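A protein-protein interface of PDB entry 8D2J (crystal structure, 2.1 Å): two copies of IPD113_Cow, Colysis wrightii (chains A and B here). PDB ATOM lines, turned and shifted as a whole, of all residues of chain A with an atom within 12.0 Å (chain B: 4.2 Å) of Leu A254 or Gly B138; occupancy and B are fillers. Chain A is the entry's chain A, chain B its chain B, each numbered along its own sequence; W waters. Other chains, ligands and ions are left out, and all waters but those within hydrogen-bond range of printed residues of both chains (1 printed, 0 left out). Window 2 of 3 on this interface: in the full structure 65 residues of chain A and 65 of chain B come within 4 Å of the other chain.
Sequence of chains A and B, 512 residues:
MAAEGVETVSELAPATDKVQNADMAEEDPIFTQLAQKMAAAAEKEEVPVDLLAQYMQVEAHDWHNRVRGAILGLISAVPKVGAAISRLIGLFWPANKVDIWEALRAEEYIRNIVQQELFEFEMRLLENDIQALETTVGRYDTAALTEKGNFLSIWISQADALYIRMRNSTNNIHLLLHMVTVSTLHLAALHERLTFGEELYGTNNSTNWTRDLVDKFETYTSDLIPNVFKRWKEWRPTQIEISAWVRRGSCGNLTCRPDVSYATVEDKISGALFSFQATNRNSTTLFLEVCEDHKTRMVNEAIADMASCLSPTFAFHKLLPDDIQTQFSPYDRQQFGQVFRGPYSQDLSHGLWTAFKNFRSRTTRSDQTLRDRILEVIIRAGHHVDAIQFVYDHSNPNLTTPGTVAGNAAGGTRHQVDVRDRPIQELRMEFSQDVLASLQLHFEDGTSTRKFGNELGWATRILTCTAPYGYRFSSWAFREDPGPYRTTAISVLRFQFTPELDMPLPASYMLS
The backbone carbonyl oxygen (O) of Trp B93 is in hydrogen-bond range of the side-chain hydroxyl (OG1) of Thr A255 (3.3 Å). OE1 of Glu B134 is in salt-bridge range of NH2 of Arg A257 (2.6 Å). The side-chain amide nitrogen of Asn A253 lies within hydrogen-bond range of the side-chain hydroxyl of Thr B135, 3.2 Å away.
The indole nitrogen (NE1) of Trp B93 lies within hydrogen-bond range of the side-chain carboxylate (OE2) of Glu B134 (3.2 Å). O of Gly B138 sits at hydrogen-bond distance from OG1 of Thr B142, 2.9 Å away. O of Ser A250 sits at hydrogen-bond distance from N of Arg A257 (3.0 Å). SG of Cys A251 is disulfide-bonded to SG of Cys A256, at 2.0 Å.
Among the printed residues, pairs that only touch across the chains: Leu A254 with Trp B93 (3.5 Å), Leu A254 with Glu B134 (3.4 Å), Leu A254 with Gly B138 (3.4 Å) and Arg A257 with Trp B93 (3.5 Å).
Of the printed residues of chain B, Asn A253 touches Thr B135 (3.2 Å). Of chain B, only Trp B93 (3.5 Å), Glu B134 (3.4 Å) and Gly B138 (3.4 Å) come within 4 Å of Leu A254. Printed residues of chain B within 4 Å of Thr A255: Trp B93 (3.3 Å). Cys A256 touches none of the printed residues of chain B. Of the printed residues of chain B, Arg A257 touches Trp B93 (3.5 Å) and Glu B134 (2.6 Å). Trp B93 touches just these residues of chain A: Leu A254, Thr A255 and Arg A257. Of the printed residues of chain A, Glu B134 touches Leu A254 and Arg A257. Of the printed residues of chain A, Thr B135 touches Asn A253 (3.2 Å). Thr B136 touches none of the printed residues of chain A. No residue of chain A comes within 4 Å of Val B137. Gly B138 touches one residue of chain A. Arg B139 touches none of the printed residues of chain A. No residue of chain A comes within 4 Å of Asp B141. No residue of chain A comes within 4 Å of Thr B142. The nearest residue of chain B that does not touch Leu A254 is Val B137 (4.05 Å).
Printed residues of chain B that touch a printed residue of chain A: Trp B93, Glu B134, Thr B135 and Gly B138. Hydrophobic or aromatic side chains of chain B within 4 Å of the printed part of chain A: Trp B93. Hydrophobic or aromatic side chains of chain A that line the printed part of chain B: Leu A254. Among the printed residues, 7 pairs touch across the chains. Among the printed residues, Asp or Glu carboxylates within 4 Å of a Lys or Arg side-chain nitrogen of the other chain: Arg A257 with Glu B134 (2.6 Å).
No position is printed for both chains.
Water W1 lies within hydrogen-bond range of the side-chain carboxylate of Asp B141 (2.7 Å) and the backbone carbonyl oxygen of Leu A254 (3.4 Å).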
ATOM      1  N   GLY A 249      18.533 -32.578 -20.369  1.00  0.00           N
ATOM      2  CA  GLY A 249      19.304 -31.508 -19.707  1.00  0.00           C
ATOM      3  C   GLY A 249      18.520 -30.207 -19.657  1.00  0.00           C
ATOM      4  O   GLY A 249      17.635 -30.019 -20.511  1.00  0.00           O
ATOM      5  N   SER A 250      18.831 -29.342 -18.689  1.00  0.00           N
ATOM      6  CA  SER A 250      18.126 -28.055 -18.442  1.00  0.00           C
ATOM      7  C   SER A 250      19.135 -26.964 -18.068  1.00  0.00           C
ATOM      8  O   SER A 250      19.863 -27.149 -17.076  1.00  0.00           O
ATOM      9  CB  SER A 250      17.079 -28.221 -17.371  1.00  0.00           C
ATOM     10  OG  SER A 250      16.335 -27.024 -17.206  1.00  0.00           O
ATOM     11  N   CYS A 251      19.171 -25.874 -18.843  1.00  0.00           N
ATOM     12  CA  CYS A 251      19.937 -24.636 -18.538  1.00  0.00           C
ATOM     13  C   CYS A 251      19.024 -23.656 -17.795  1.00  0.00           C
ATOM     14  O   CYS A 251      18.003 -23.245 -18.379  1.00  0.00           O
ATOM     15  CB  CYS A 251      20.486 -23.986 -19.802  1.00  0.00           C
ATOM     16  SG  CYS A 251      21.737 -24.991 -20.642  1.00  0.00           S
ATOM     17  N   GLY A 252      19.374 -23.325 -16.548  1.00  0.00           N
ATOM     18  CA  GLY A 252      18.636 -22.375 -15.693  1.00  0.00           C
ATOM     19  C   GLY A 252      19.580 -21.402 -15.011  1.00  0.00           C
ATOM     20  O   GLY A 252      20.603 -21.042 -15.628  1.00  0.00           O
ATOM     21  N   ASN A 253      19.246 -20.992 -13.784  1.00  0.00           N
ATOM     22  CA  ASN A 253      20.082 -20.104 -12.933  1.00  0.00           C
ATOM     23  C   ASN A 253      21.124 -20.959 -12.203  1.00  0.00           C
ATOM     24  O   ASN A 253      20.728 -21.671 -11.257  1.00  0.00           O
ATOM     25  CB  ASN A 253      19.237 -19.312 -11.930  1.00  0.00           C
ATOM     26  CG  ASN A 253      18.100 -18.544 -12.572  1.00  0.00           C
ATOM     27  OD1 ASN A 253      18.205 -18.106 -13.715  1.00  0.00           O
ATOM     28  ND2 ASN A 253      17.009 -18.374 -11.842  1.00  0.00           N
ATOM     29  N   LEU A 254      22.382 -20.918 -12.667  1.00  0.00           N
ATOM     30  CA  LEU A 254      23.611 -21.421 -11.983  1.00  0.00           C
ATOM     31  C   LEU A 254      24.444 -22.276 -12.949  1.00  0.00           C
ATOM     32  O   LEU A 254      25.666 -22.043 -13.013  1.00  0.00           O
ATOM     33  CB  LEU A 254      23.249 -22.198 -10.709  1.00  0.00           C
ATOM     34  CG  LEU A 254      24.393 -22.930 -10.005  1.00  0.00           C
ATOM     35  CD1 LEU A 254      25.509 -21.976  -9.607  1.00  0.00           C
ATOM     36  CD2 LEU A 254      23.875 -23.670  -8.783  1.00  0.00           C
ATOM     37  N   THR A 255      23.826 -23.224 -13.667  1.00  0.00           N
ATOM     38  CA  THR A 255      24.538 -24.181 -14.561  1.00  0.00           C
ATOM     39  C   THR A 255      23.640 -24.661 -15.709  1.00  0.00           C
ATOM     40  O   THR A 255      22.422 -24.390 -15.680  1.00  0.00           O
ATOM     41  CB  THR A 255      25.052 -25.394 -13.775  1.00  0.00           C
ATOM     42  OG1 THR A 255      26.036 -26.052 -14.576  1.00  0.00           O
ATOM     43  CG2 THR A 255      23.960 -26.373 -13.399  1.00  0.00           C
ATOM     44  N   CYS A 256      24.249 -25.361 -16.671  1.00  0.00           N
ATOM     45  CA  CYS A 256      23.579 -26.175 -17.719  1.00  0.00           C
ATOM     46  C   CYS A 256      23.725 -27.656 -17.356  1.00  0.00           C
ATOM     47  O   CYS A 256      24.821 -28.213 -17.574  1.00  0.00           O
ATOM     48  CB  CYS A 256      24.164 -25.891 -19.098  1.00  0.00           C
ATOM     49  SG  CYS A 256      23.509 -24.380 -19.852  1.00  0.00           S
ATOM     50  N   ARG A 257      22.668 -28.248 -16.788  1.00  0.00           N
ATOM     51  CA  ARG A 257      22.623 -29.675 -16.370  1.00  0.00           C
ATOM     52  C   ARG A 257      22.569 -30.550 -17.618  1.00  0.00           C
ATOM     53  O   ARG A 257      21.810 -30.266 -18.542  1.00  0.00           O
ATOM     54  CB  ARG A 257      21.415 -29.935 -15.463  1.00  0.00           C
ATOM     55  CG  ARG A 257      21.464 -29.186 -14.139  1.00  0.00           C
ATOM     56  CD  ARG A 257      20.205 -29.383 -13.317  1.00  0.00           C
ATOM     57  NE  ARG A 257      20.035 -28.320 -12.332  1.00  0.00           N
ATOM     58  CZ  ARG A 257      20.579 -28.300 -11.117  1.00  0.00           C
ATOM     59  NH1 ARG A 257      21.345 -29.294 -10.702  1.00  0.00           N
ATOM     60  NH2 ARG A 257      20.355 -27.276 -10.313  1.00  0.00           N
ATOM     61  N   PRO A 258      23.364 -31.642 -17.686  1.00  0.00           N
ATOM     62  CA  PRO A 258      23.400 -32.493 -18.874  1.00  0.00           C
ATOM     63  C   PRO A 258      22.215 -33.465 -18.956  1.00  0.00           C
ATOM     64  O   PRO A 258      21.561 -33.692 -17.947  1.00  0.00           O
ATOM     65  CB  PRO A 258      24.709 -33.271 -18.675  1.00  0.00           C
ATOM     66  CG  PRO A 258      24.803 -33.429 -17.173  1.00  0.00           C
ATOM     67  CD  PRO A 258      24.254 -32.130 -16.619  1.00  0.00           C
ATOM     68  N   TRP B  93      27.863 -28.727  -9.260  1.00  0.00           N
ATOM     69  CA  TRP B  93      27.042 -28.537 -10.486  1.00  0.00           C
ATOM     70  C   TRP B  93      27.937 -28.549 -11.720  1.00  0.00           C
ATOM     71  O   TRP B  93      28.035 -27.551 -12.428  1.00  0.00           O
ATOM     72  CB  TRP B  93      26.234 -27.239 -10.384  1.00  0.00           C
ATOM     73  CG  TRP B  93      25.299 -27.216  -9.215  1.00  0.00           C
ATOM     74  CD1 TRP B  93      24.059 -27.776  -9.142  1.00  0.00           C
ATOM     75  CD2 TRP B  93      25.544 -26.615  -7.933  1.00  0.00           C
ATOM     76  NE1 TRP B  93      23.509 -27.557  -7.907  1.00  0.00           N
ATOM     77  CE2 TRP B  93      24.395 -26.845  -7.145  1.00  0.00           C
ATOM     78  CE3 TRP B  93      26.609 -25.894  -7.382  1.00  0.00           C
ATOM     79  CZ2 TRP B  93      24.293 -26.385  -5.832  1.00  0.00           C
ATOM     80  CZ3 TRP B  93      26.505 -25.437  -6.087  1.00  0.00           C
ATOM     81  CH2 TRP B  93      25.361 -25.681  -5.326  1.00  0.00           C
ATOM     82  N   GLU B 134      20.256 -21.939  -5.211  1.00  0.00           N
ATOM     83  CA  GLU B 134      21.151 -22.223  -6.365  1.00  0.00           C
ATOM     84  C   GLU B 134      21.257 -20.979  -7.255  1.00  0.00           C
ATOM     85  O   GLU B 134      22.372 -20.707  -7.735  1.00  0.00           O
ATOM     86  CB  GLU B 134      20.653 -23.440  -7.145  1.00  0.00           C
ATOM     87  CG  GLU B 134      20.981 -24.751  -6.457  1.00  0.00           C
ATOM     88  CD  GLU B 134      20.454 -25.989  -7.156  1.00  0.00           C
ATOM     89  OE1 GLU B 134      19.853 -25.849  -8.237  1.00  0.00           O
ATOM     90  OE2 GLU B 134      20.644 -27.091  -6.614  1.00  0.00           O
ATOM     91  N   THR B 135      20.148 -20.260  -7.462  1.00  0.00           N
ATOM     92  CA  THR B 135      20.101 -18.981  -8.226  1.00  0.00           C
ATOM     93  C   THR B 135      21.073 -17.984  -7.584  1.00  0.00           C
ATOM     94  O   THR B 135      21.873 -17.379  -8.328  1.00  0.00           O
ATOM     95  CB  THR B 135      18.674 -18.418  -8.304  1.00  0.00           C
ATOM     96  OG1 THR B 135      17.848 -19.381  -8.960  1.00  0.00           O
ATOM     97  CG2 THR B 135      18.588 -17.102  -9.046  1.00  0.00           C
ATOM     98  N   THR B 136      21.011 -17.840  -6.255  1.00  0.00           N
ATOM     99  CA  THR B 136      21.844 -16.904  -5.451  1.00  0.00           C
ATOM    100  C   THR B 136      23.329 -17.270  -5.578  1.00  0.00           C
ATOM    101  O   THR B 136      24.150 -16.340  -5.698  1.00  0.00           O
ATOM    102  CB  THR B 136      21.407 -16.891  -3.981  1.00  0.00           C
ATOM    103  OG1 THR B 136      19.993 -16.686  -3.944  1.00  0.00           O
ATOM    104  CG2 THR B 136      22.106 -15.821  -3.170  1.00  0.00           C
ATOM    105  N   VAL B 137      23.655 -18.566  -5.541  1.00  0.00           N
ATOM    106  CA  VAL B 137      25.053 -19.091  -5.633  1.00  0.00           C
ATOM    107  C   VAL B 137      25.637 -18.701  -6.998  1.00  0.00           C
ATOM    108  O   VAL B 137      26.792 -18.229  -7.034  1.00  0.00           O
ATOM    109  CB  VAL B 137      25.103 -20.615  -5.406  1.00  0.00           C
ATOM    110  CG1 VAL B 137      26.463 -21.204  -5.751  1.00  0.00           C
ATOM    111  CG2 VAL B 137      24.713 -20.988  -3.985  1.00  0.00           C
ATOM    112  N   GLY B 138      24.869 -18.905  -8.072  1.00  0.00           N
ATOM    113  CA  GLY B 138      25.249 -18.541  -9.452  1.00  0.00           C
ATOM    114  C   GLY B 138      25.430 -17.041  -9.605  1.00  0.00           C
ATOM    115  O   GLY B 138      26.367 -16.630 -10.314  1.00  0.00           O
ATOM    116  N   ARG B 139      24.564 -16.254  -8.959  1.00  0.00           N
ATOM    117  CA  ARG B 139      24.602 -14.767  -8.986  1.00  0.00           C
ATOM    118  C   ARG B 139      25.873 -14.278  -8.279  1.00  0.00           C
ATOM    119  O   ARG B 139      26.525 -13.370  -8.821  1.00  0.00           O
ATOM    120  CB  ARG B 139      23.331 -14.179  -8.365  1.00  0.00           C
ATOM    121  CG  ARG B 139      22.130 -14.193  -9.301  1.00  0.00           C
ATOM    122  CD  ARG B 139      20.825 -13.892  -8.588  1.00  0.00           C
ATOM    123  NE  ARG B 139      19.718 -13.724  -9.521  1.00  0.00           N
ATOM    124  CZ  ARG B 139      18.435 -13.623  -9.179  1.00  0.00           C
ATOM    125  NH1 ARG B 139      18.068 -13.672  -7.908  1.00  0.00           N
ATOM    126  NH2 ARG B 139      17.517 -13.474 -10.118  1.00  0.00           N
ATOM    127  N   TYR B 140      26.223 -14.870  -7.129  1.00  0.00           N
ATOM    128  CA  TYR B 140      27.471 -14.561  -6.383  1.00  0.00           C
ATOM    129  C   TYR B 140      28.690 -14.833  -7.273  1.00  0.00           C
ATOM    130  O   TYR B 140      29.610 -13.996  -7.304  1.00  0.00           O
ATOM    131  CB  TYR B 140      27.586 -15.373  -5.089  1.00  0.00           C
ATOM    132  CG  TYR B 140      28.859 -15.091  -4.333  1.00  0.00           C
ATOM    133  CD1 TYR B 140      28.925 -14.062  -3.408  1.00  0.00           C
ATOM    134  CD2 TYR B 140      30.017 -15.812  -4.584  1.00  0.00           C
ATOM    135  CE1 TYR B 140      30.098 -13.773  -2.731  1.00  0.00           C
ATOM    136  CE2 TYR B 140      31.199 -15.536  -3.916  1.00  0.00           C
ATOM    137  CZ  TYR B 140      31.239 -14.514  -2.984  1.00  0.00           C
ATOM    138  OH  TYR B 140      32.395 -14.226  -2.324  1.00  0.00           O
ATOM    139  N   ASP B 141      28.693 -15.977  -7.963  1.00  0.00           N
ATOM    140  CA  ASP B 141      29.846 -16.488  -8.754  1.00  0.00           C
ATOM    141  C   ASP B 141      30.109 -15.570  -9.955  1.00  0.00           C
ATOM    142  O   ASP B 141      31.296 -15.345 -10.265  1.00  0.00           O
ATOM    143  CB  ASP B 141      29.601 -17.933  -9.196  1.00  0.00           C
ATOM    144  CG  ASP B 141      30.799 -18.598  -9.854  1.00  0.00           C
ATOM    145  OD1 ASP B 141      31.923 -18.418  -9.349  1.00  0.00           O
ATOM    146  OD2 ASP B 141      30.595 -19.291 -10.872  1.00  0.00           O
ATOM    147  N   THR B 142      29.048 -15.064 -10.596  1.00  0.00           N
ATOM    148  CA  THR B 142      29.098 -14.282 -11.864  1.00  0.00           C
ATOM    149  C   THR B 142      29.201 -12.777 -11.581  1.00  0.00           C
ATOM    150  O   THR B 142      29.662 -12.050 -12.485  1.00  0.00           O
ATOM    151  CB  THR B 142      27.867 -14.556 -12.738  1.00  0.00           C
ATOM    152  OG1 THR B 142      26.702 -14.252 -11.969  1.00  0.00           O
ATOM    153  CG2 THR B 142      27.798 -15.983 -13.235  1.00  0.00           C
HETATM  154  O   HOH W   1      28.285 -20.151 -11.995  1.00  0.00           O
